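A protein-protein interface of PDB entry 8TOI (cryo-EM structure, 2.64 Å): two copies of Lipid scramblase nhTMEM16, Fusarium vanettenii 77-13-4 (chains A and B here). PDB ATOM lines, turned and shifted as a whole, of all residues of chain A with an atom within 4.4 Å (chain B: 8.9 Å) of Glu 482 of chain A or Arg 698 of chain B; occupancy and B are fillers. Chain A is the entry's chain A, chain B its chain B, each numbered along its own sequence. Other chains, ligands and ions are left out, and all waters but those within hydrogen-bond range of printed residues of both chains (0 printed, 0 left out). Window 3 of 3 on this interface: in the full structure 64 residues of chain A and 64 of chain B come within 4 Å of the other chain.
A ring nitrogen (ND1) of His 480 of chain A is in hydrogen-bond range of the side-chain carboxylate of Glu 483 of chain A, 2.9 Å away.
The guanidinium group (NH1) of Arg 58 of chain A is in salt-bridge range of the side-chain carboxylate (OE2) of Glu 56 of chain A, at 2.5 Å.
The backbone carbonyl oxygen (O) of Met 694 of chain B lies within hydrogen-bond range of the guanidinium group (NE) of Arg 698 of chain B (2.9 Å).
The guanidinium group of Arg 58 of chain A is in salt-bridge range of the side-chain carboxylate of Glu 483 of chain A.
Of the 8 printed residues of chain A, 5 touch a printed residue of chain B.
Along chain A the printed residues that touch a printed residue of chain B span positions 56 to 483.
Among the printed residues, Asp or Glu carboxylates within 4 Å of a Lys or Arg side-chain nitrogen of the other chain: Glu 482 of chain A with Arg 698 of chain B (3.3 Å).
Among the printed residues, merely in contact across the chains: Glu 483 of chain A with Phe 695 of chain B, Arg 58 of chain A with Phe 695 of chain B, Glu 56 of chain A with Arg 698 of chain B, Glu 56 of chain A with Trp 696 of chain B and Arg 58 of chain A with Met 712 of chain B.
Printed residues of chain B within 4 Å of Glu 56 of chain A: Phe 695 (3.1 Å), Trp 696 (3.7 Å), Arg 698 (3.4 Å) and Gln 699 (3.4 Å).
Of chain B, only Arg 698 comes within 4 Å of Glu 482 of chain A.
Leu 676 of chain B touches none of the printed residues of chain A.
Of chain A, only Glu 56, Arg 58, His 480 and Glu 482 come within 4 Å of Arg 698 of chain B.
Of the printed residues of chain A, Gln 699 of chain B touches Glu 56.
Glu 704 of chain B touches none of the printed residues of chain A.
The nearest printed residue of chain A that does not touch Phe 695 of chain B is His 480 of chain A (6.7 Å).
No position is printed for both chains.
Of the 10 pairs that touch across the chains among the printed residues, none has its exchanged pair printed and touching as well.
OE1 of Glu 56 of chain A sits close to O of Gln 699 of chain B (3.4 Å).
OE2 of Glu 56 of chain A lies close to O of Phe 695 of chain B, at 3.1 Å.
The guanidinium group (NH2) of Arg 58 of chain A lies close to the guanidinium group (NE) of Arg 698 of chain B (3.5 Å).
NH1 of Arg 698 of chain B sits at hydrogen-bond distance from ND1 of His 480 of chain A.
The side-chain carboxylate of Glu 482 of chain A lies within salt-bridge range of the guanidinium group of Arg 698 of chain B, at 3.3 Å.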
ATOM      1  N   GLU A  56     -16.988  -4.444  -9.953  1.00  0.00           N
ATOM      2  CA  GLU A  56     -17.734  -5.174 -10.973  1.00  0.00           C
ATOM      3  C   GLU A  56     -18.721  -6.085 -10.260  1.00  0.00           C
ATOM      4  O   GLU A  56     -18.309  -6.971  -9.506  1.00  0.00           O
ATOM      5  CB  GLU A  56     -16.794  -5.967 -11.871  1.00  0.00           C
ATOM      6  CG  GLU A  56     -17.499  -6.735 -12.963  1.00  0.00           C
ATOM      7  CD  GLU A  56     -17.756  -5.889 -14.192  1.00  0.00           C
ATOM      8  OE1 GLU A  56     -17.158  -4.798 -14.300  1.00  0.00           O
ATOM      9  OE2 GLU A  56     -18.554  -6.314 -15.053  1.00  0.00           O
ATOM     10  N   ARG A  58     -21.608  -8.991 -10.030  1.00  0.00           N
ATOM     11  CA  ARG A  58     -21.981 -10.230 -10.697  1.00  0.00           C
ATOM     12  C   ARG A  58     -22.996 -10.965  -9.838  1.00  0.00           C
ATOM     13  O   ARG A  58     -23.250 -10.602  -8.687  1.00  0.00           O
ATOM     14  CB  ARG A  58     -20.766 -11.127 -10.962  1.00  0.00           C
ATOM     15  CG  ARG A  58     -19.891 -10.679 -12.114  1.00  0.00           C
ATOM     16  CD  ARG A  58     -20.562 -10.906 -13.450  1.00  0.00           C
ATOM     17  NE  ARG A  58     -19.611 -10.765 -14.544  1.00  0.00           N
ATOM     18  CZ  ARG A  58     -19.270  -9.608 -15.095  1.00  0.00           C
ATOM     19  NH1 ARG A  58     -19.817  -8.469 -14.704  1.00  0.00           N
ATOM     20  NH2 ARG A  58     -18.361  -9.596 -16.066  1.00  0.00           N
ATOM     21  N   ASP A 479     -24.340 -16.099 -17.011  1.00  0.00           N
ATOM     22  CA  ASP A 479     -22.958 -15.773 -16.630  1.00  0.00           C
ATOM     23  C   ASP A 479     -22.087 -15.402 -17.831  1.00  0.00           C
ATOM     24  O   ASP A 479     -20.894 -15.714 -17.857  1.00  0.00           O
ATOM     25  CB  ASP A 479     -22.311 -16.909 -15.831  1.00  0.00           C
ATOM     26  CG  ASP A 479     -23.033 -17.190 -14.530  1.00  0.00           C
ATOM     27  OD1 ASP A 479     -24.069 -16.541 -14.272  1.00  0.00           O
ATOM     28  OD2 ASP A 479     -22.566 -18.059 -13.765  1.00  0.00           O
ATOM     29  N   HIS A 480     -22.695 -14.774 -18.842  1.00  0.00           N
ATOM     30  CA  HIS A 480     -22.054 -14.136 -19.993  1.00  0.00           C
ATOM     31  C   HIS A 480     -21.282 -15.097 -20.897  1.00  0.00           C
ATOM     32  O   HIS A 480     -20.545 -14.637 -21.772  1.00  0.00           O
ATOM     33  CB  HIS A 480     -21.134 -12.985 -19.558  1.00  0.00           C
ATOM     34  CG  HIS A 480     -21.868 -11.811 -18.990  1.00  0.00           C
ATOM     35  ND1 HIS A 480     -21.225 -10.757 -18.377  1.00  0.00           N
ATOM     36  CD2 HIS A 480     -23.190 -11.522 -18.944  1.00  0.00           C
ATOM     37  CE1 HIS A 480     -22.119  -9.871 -17.976  1.00  0.00           C
ATOM     38  NE2 HIS A 480     -23.320 -10.312 -18.309  1.00  0.00           N
ATOM     39  N   GLU A 481     -21.427 -16.416 -20.694  1.00  0.00           N
ATOM     40  CA  GLU A 481     -20.957 -17.539 -21.542  1.00  0.00           C
ATOM     41  C   GLU A 481     -19.477 -17.461 -21.965  1.00  0.00           C
ATOM     42  O   GLU A 481     -19.074 -18.132 -22.920  1.00  0.00           O
ATOM     43  CB  GLU A 481     -21.847 -17.767 -22.784  1.00  0.00           C
ATOM     44  CG  GLU A 481     -21.886 -16.700 -23.886  1.00  0.00           C
ATOM     45  CD  GLU A 481     -23.042 -15.724 -23.735  1.00  0.00           C
ATOM     46  OE1 GLU A 481     -23.699 -15.718 -22.675  1.00  0.00           O
ATOM     47  OE2 GLU A 481     -23.293 -14.956 -24.688  1.00  0.00           O
ATOM     48  N   GLU A 482     -18.638 -16.678 -21.282  1.00  0.00           N
ATOM     49  CA  GLU A 482     -17.191 -16.817 -21.411  1.00  0.00           C
ATOM     50  C   GLU A 482     -16.474 -16.631 -20.080  1.00  0.00           C
ATOM     51  O   GLU A 482     -15.238 -16.634 -20.050  1.00  0.00           O
ATOM     52  CB  GLU A 482     -16.604 -15.848 -22.449  1.00  0.00           C
ATOM     53  CG  GLU A 482     -16.729 -14.376 -22.111  1.00  0.00           C
ATOM     54  CD  GLU A 482     -17.777 -13.678 -22.953  1.00  0.00           C
ATOM     55  OE1 GLU A 482     -18.479 -14.371 -23.719  1.00  0.00           O
ATOM     56  OE2 GLU A 482     -17.898 -12.440 -22.852  1.00  0.00           O
ATOM     57  N   GLU A 483     -17.214 -16.466 -18.984  1.00  0.00           N
ATOM     58  CA  GLU A 483     -16.626 -16.336 -17.658  1.00  0.00           C
ATOM     59  C   GLU A 483     -17.371 -17.186 -16.637  1.00  0.00           C
ATOM     60  O   GLU A 483     -17.222 -16.968 -15.430  1.00  0.00           O
ATOM     61  CB  GLU A 483     -16.605 -14.870 -17.220  1.00  0.00           C
ATOM     62  CG  GLU A 483     -17.979 -14.228 -17.157  1.00  0.00           C
ATOM     63  CD  GLU A 483     -17.923 -12.717 -17.251  1.00  0.00           C
ATOM     64  OE1 GLU A 483     -16.832 -12.177 -17.532  1.00  0.00           O
ATOM     65  OE2 GLU A 483     -18.970 -12.069 -17.048  1.00  0.00           O
ATOM     66  N   ALA A 484     -18.169 -18.151 -17.104  1.00  0.00           N
ATOM     67  CA  ALA A 484     -18.979 -18.966 -16.205  1.00  0.00           C
ATOM     68  C   ALA A 484     -18.127 -19.907 -15.365  1.00  0.00           C
ATOM     69  O   ALA A 484     -18.521 -20.257 -14.247  1.00  0.00           O
ATOM     70  CB  ALA A 484     -20.012 -19.760 -17.003  1.00  0.00           C
ATOM     71  N   LEU B 676      -9.479   2.977 -17.214  1.00  0.00           N
ATOM     72  CA  LEU B 676     -10.112   1.925 -18.001  1.00  0.00           C
ATOM     73  C   LEU B 676     -10.146   2.281 -19.484  1.00  0.00           C
ATOM     74  O   LEU B 676     -10.113   1.389 -20.338  1.00  0.00           O
ATOM     75  CB  LEU B 676     -11.514   1.651 -17.459  1.00  0.00           C
ATOM     76  CG  LEU B 676     -11.488   0.946 -16.096  1.00  0.00           C
ATOM     77  CD1 LEU B 676     -12.824   1.059 -15.379  1.00  0.00           C
ATOM     78  CD2 LEU B 676     -11.049  -0.506 -16.207  1.00  0.00           C
ATOM     79  N   THR B 690      -8.011 -11.049 -23.901  1.00  0.00           N
ATOM     80  CA  THR B 690      -9.284 -10.407 -24.233  1.00  0.00           C
ATOM     81  C   THR B 690     -10.369 -10.591 -23.164  1.00  0.00           C
ATOM     82  O   THR B 690     -11.005  -9.584 -22.808  1.00  0.00           O
ATOM     83  CB  THR B 690      -9.751 -10.853 -25.626  1.00  0.00           C
ATOM     84  N   PRO B 691     -10.646 -11.796 -22.612  1.00  0.00           N
ATOM     85  CA  PRO B 691     -11.631 -11.849 -21.514  1.00  0.00           C
ATOM     86  C   PRO B 691     -11.155 -11.184 -20.235  1.00  0.00           C
ATOM     87  O   PRO B 691     -11.998 -10.726 -19.454  1.00  0.00           O
ATOM     88  CB  PRO B 691     -11.860 -13.351 -21.309  1.00  0.00           C
ATOM     89  CG  PRO B 691     -10.616 -13.965 -21.744  1.00  0.00           C
ATOM     90  CD  PRO B 691     -10.220 -13.177 -22.947  1.00  0.00           C
ATOM     91  N   GLU B 692      -9.835 -11.087 -20.030  1.00  0.00           N
ATOM     92  CA  GLU B 692      -9.277 -10.326 -18.916  1.00  0.00           C
ATOM     93  C   GLU B 692      -9.680  -8.858 -18.992  1.00  0.00           C
ATOM     94  O   GLU B 692     -10.039  -8.250 -17.977  1.00  0.00           O
ATOM     95  CB  GLU B 692      -7.752 -10.462 -18.922  1.00  0.00           C
ATOM     96  CG  GLU B 692      -7.020  -9.568 -17.936  1.00  0.00           C
ATOM     97  CD  GLU B 692      -7.123 -10.063 -16.513  1.00  0.00           C
ATOM     98  OE1 GLU B 692      -7.264 -11.288 -16.325  1.00  0.00           O
ATOM     99  OE2 GLU B 692      -7.059  -9.229 -15.586  1.00  0.00           O
ATOM    100  N   GLU B 693      -9.635  -8.275 -20.192  1.00  0.00           N
ATOM    101  CA  GLU B 693     -10.092  -6.901 -20.356  1.00  0.00           C
ATOM    102  C   GLU B 693     -11.613  -6.808 -20.295  1.00  0.00           C
ATOM    103  O   GLU B 693     -12.157  -5.982 -19.553  1.00  0.00           O
ATOM    104  CB  GLU B 693      -9.571  -6.329 -21.672  1.00  0.00           C
ATOM    105  N   MET B 694     -12.319  -7.673 -21.029  1.00  0.00           N
ATOM    106  CA  MET B 694     -13.770  -7.546 -21.145  1.00  0.00           C
ATOM    107  C   MET B 694     -14.530  -7.980 -19.899  1.00  0.00           C
ATOM    108  O   MET B 694     -15.754  -7.810 -19.858  1.00  0.00           O
ATOM    109  CB  MET B 694     -14.290  -8.325 -22.355  1.00  0.00           C
ATOM    110  CG  MET B 694     -13.656  -7.925 -23.673  1.00  0.00           C
ATOM    111  SD  MET B 694     -13.505  -6.137 -23.843  1.00  0.00           S
ATOM    112  CE  MET B 694     -14.977  -5.762 -24.789  1.00  0.00           C
ATOM    113  N   PHE B 695     -13.858  -8.555 -18.897  1.00  0.00           N
ATOM    114  CA  PHE B 695     -14.505  -8.723 -17.602  1.00  0.00           C
ATOM    115  C   PHE B 695     -14.779  -7.378 -16.942  1.00  0.00           C
ATOM    116  O   PHE B 695     -15.793  -7.222 -16.254  1.00  0.00           O
ATOM    117  CB  PHE B 695     -13.644  -9.597 -16.694  1.00  0.00           C
ATOM    118  CG  PHE B 695     -14.217  -9.797 -15.323  1.00  0.00           C
ATOM    119  CD1 PHE B 695     -15.320 -10.609 -15.134  1.00  0.00           C
ATOM    120  CD2 PHE B 695     -13.649  -9.180 -14.221  1.00  0.00           C
ATOM    121  CE1 PHE B 695     -15.851 -10.801 -13.875  1.00  0.00           C
ATOM    122  CE2 PHE B 695     -14.175  -9.368 -12.958  1.00  0.00           C
ATOM    123  CZ  PHE B 695     -15.277 -10.178 -12.787  1.00  0.00           C
ATOM    124  N   TRP B 696     -13.896  -6.397 -17.142  1.00  0.00           N
ATOM    125  CA  TRP B 696     -14.042  -5.083 -16.534  1.00  0.00           C
ATOM    126  C   TRP B 696     -14.545  -4.016 -17.501  1.00  0.00           C
ATOM    127  O   TRP B 696     -15.174  -3.053 -17.055  1.00  0.00           O
ATOM    128  CB  TRP B 696     -12.706  -4.622 -15.940  1.00  0.00           C
ATOM    129  CG  TRP B 696     -12.161  -5.540 -14.895  1.00  0.00           C
ATOM    130  CD1 TRP B 696     -11.297  -6.573 -15.089  1.00  0.00           C
ATOM    131  CD2 TRP B 696     -12.442  -5.511 -13.492  1.00  0.00           C
ATOM    132  NE1 TRP B 696     -11.020  -7.191 -13.896  1.00  0.00           N
ATOM    133  CE2 TRP B 696     -11.714  -6.559 -12.899  1.00  0.00           C
ATOM    134  CE3 TRP B 696     -13.242  -4.704 -12.681  1.00  0.00           C
ATOM    135  CZ2 TRP B 696     -11.756  -6.818 -11.534  1.00  0.00           C
ATOM    136  CZ3 TRP B 696     -13.284  -4.963 -11.324  1.00  0.00           C
ATOM    137  CH2 TRP B 696     -12.546  -6.010 -10.766  1.00  0.00           C
ATOM    138  N   GLN B 697     -14.290  -4.159 -18.802  1.00  0.00           N
ATOM    139  CA  GLN B 697     -14.648  -3.126 -19.766  1.00  0.00           C
ATOM    140  C   GLN B 697     -16.125  -3.088 -20.123  1.00  0.00           C
ATOM    141  O   GLN B 697     -16.547  -2.151 -20.809  1.00  0.00           O
ATOM    142  CB  GLN B 697     -13.844  -3.277 -21.063  1.00  0.00           C
ATOM    143  CG  GLN B 697     -12.368  -3.042 -20.907  1.00  0.00           C
ATOM    144  CD  GLN B 697     -12.080  -1.635 -20.452  1.00  0.00           C
ATOM    145  OE1 GLN B 697     -11.666  -1.412 -19.320  1.00  0.00           O
ATOM    146  NE2 GLN B 697     -12.352  -0.670 -21.316  1.00  0.00           N
ATOM    147  N   ARG B 698     -16.919  -4.072 -19.704  1.00  0.00           N
ATOM    148  CA  ARG B 698     -18.341  -4.010 -20.007  1.00  0.00           C
ATOM    149  C   ARG B 698     -19.070  -2.990 -19.143  1.00  0.00           C
ATOM    150  O   ARG B 698     -20.084  -2.435 -19.585  1.00  0.00           O
ATOM    151  CB  ARG B 698     -18.987  -5.391 -19.853  1.00  0.00           C
ATOM    152  CG  ARG B 698     -18.990  -5.964 -18.444  1.00  0.00           C
ATOM    153  CD  ARG B 698     -19.417  -7.414 -18.453  1.00  0.00           C
ATOM    154  NE  ARG B 698     -18.528  -8.236 -19.264  1.00  0.00           N
ATOM    155  CZ  ARG B 698     -18.925  -8.987 -20.280  1.00  0.00           C
ATOM    156  NH1 ARG B 698     -20.192  -9.020 -20.660  1.00  0.00           N
ATOM    157  NH2 ARG B 698     -18.030  -9.717 -20.936  1.00  0.00           N
ATOM    158  N   GLN B 699     -18.583  -2.737 -17.929  1.00  0.00           N
ATOM    159  CA  GLN B 699     -19.202  -1.797 -17.000  1.00  0.00           C
ATOM    160  C   GLN B 699     -18.075  -1.037 -16.322  1.00  0.00           C
ATOM    161  O   GLN B 699     -17.317  -1.622 -15.544  1.00  0.00           O
ATOM    162  CB  GLN B 699     -20.061  -2.533 -15.965  1.00  0.00           C
ATOM    163  CG  GLN B 699     -21.277  -3.213 -16.556  1.00  0.00           C
ATOM    164  CD  GLN B 699     -22.099  -3.953 -15.543  1.00  0.00           C
ATOM    165  OE1 GLN B 699     -23.152  -4.505 -15.854  1.00  0.00           O
ATOM    166  NE2 GLN B 699     -21.639  -3.933 -14.301  1.00  0.00           N
ATOM    167  N   ARG B 700     -17.974   0.250 -16.595  1.00  0.00           N
ATOM    168  CA  ARG B 700     -16.797   0.986 -16.150  1.00  0.00           C
ATOM    169  C   ARG B 700     -17.140   2.207 -15.317  1.00  0.00           C
ATOM    170  O   ARG B 700     -16.282   2.704 -14.585  1.00  0.00           O
ATOM    171  CB  ARG B 700     -15.951   1.413 -17.364  1.00  0.00           C
ATOM    172  CG  ARG B 700     -16.630   2.423 -18.275  1.00  0.00           C
ATOM    173  CD  ARG B 700     -15.793   2.712 -19.510  1.00  0.00           C
ATOM    174  NE  ARG B 700     -16.385   3.753 -20.343  1.00  0.00           N
ATOM    175  CZ  ARG B 700     -17.288   3.537 -21.289  1.00  0.00           C
ATOM    176  NH1 ARG B 700     -17.718   2.319 -21.572  1.00  0.00           N
ATOM    177  NH2 ARG B 700     -17.771   4.573 -21.972  1.00  0.00           N
ATOM    178  N   GLY B 701     -18.369   2.702 -15.409  1.00  0.00           N
ATOM    179  CA  GLY B 701     -18.771   3.876 -14.675  1.00  0.00           C
ATOM    180  C   GLY B 701     -19.319   3.531 -13.306  1.00  0.00           C
ATOM    181  O   GLY B 701     -19.323   2.382 -12.861  1.00  0.00           O
ATOM    182  N   GLU B 704     -23.955   2.818 -13.917  1.00  0.00           N
ATOM    183  CA  GLU B 704     -24.435   1.606 -14.583  1.00  0.00           C
ATOM    184  C   GLU B 704     -24.199   0.348 -13.754  1.00  0.00           C
ATOM    185  O   GLU B 704     -24.978  -0.604 -13.872  1.00  0.00           O
ATOM    186  CB  GLU B 704     -23.796   1.474 -15.970  1.00  0.00           C
ATOM    187  CG  GLU B 704     -22.329   1.093 -15.983  1.00  0.00           C
ATOM    188  CD  GLU B 704     -21.440   2.254 -16.370  1.00  0.00           C
ATOM    189  OE1 GLU B 704     -21.832   3.414 -16.117  1.00  0.00           O
ATOM    190  OE2 GLU B 704     -20.351   2.012 -16.933  1.00  0.00           O
ATOM    191  N   THR B 705     -23.204   0.366 -12.861  1.00  0.00           N
ATOM    192  CA  THR B 705     -23.079  -0.675 -11.849  1.00  0.00           C
ATOM    193  C   THR B 705     -24.292  -0.689 -10.924  1.00  0.00           C
ATOM    194  O   THR B 705     -24.789  -1.764 -10.570  1.00  0.00           O
ATOM    195  CB  THR B 705     -21.790  -0.472 -11.053  1.00  0.00           C
ATOM    196  OG1 THR B 705     -20.687  -0.353 -11.959  1.00  0.00           O
ATOM    197  CG2 THR B 705     -21.533  -1.647 -10.125  1.00  0.00           C
ATOM    198  N   ILE B 708     -27.365  -2.101 -12.966  1.00  0.00           N
ATOM    199  CA  ILE B 708     -27.299  -3.536 -13.246  1.00  0.00           C
ATOM    200  C   ILE B 708     -27.324  -4.352 -11.950  1.00  0.00           C
ATOM    201  O   ILE B 708     -27.878  -5.459 -11.924  1.00  0.00           O
ATOM    202  CB  ILE B 708     -26.099  -3.863 -14.157  1.00  0.00           C
ATOM    203  CG1 ILE B 708     -26.242  -3.089 -15.469  1.00  0.00           C
ATOM    204  CG2 ILE B 708     -26.039  -5.345 -14.507  1.00  0.00           C
ATOM    205  CD1 ILE B 708     -27.496  -3.436 -16.261  1.00  0.00           C
ATOM    206  N   MET B 712     -30.124  -7.102 -11.289  1.00  0.00           N
ATOM    207  CA  MET B 712     -29.807  -8.448 -10.822  1.00  0.00           C
ATOM    208  C   MET B 712     -30.580  -8.789  -9.557  1.00  0.00           C
ATOM    209  O   MET B 712     -30.996  -9.938  -9.370  1.00  0.00           O
ATOM    210  CB  MET B 712     -28.304  -8.586 -10.579  1.00  0.00           C
ATOM    211  CG  MET B 712     -27.466  -8.769 -11.831  1.00  0.00           C
ATOM    212  SD  MET B 712     -25.701  -8.702 -11.469  1.00  0.00           S
ATOM    213  CE  MET B 712     -25.005  -9.076 -13.075  1.00  0.00           C
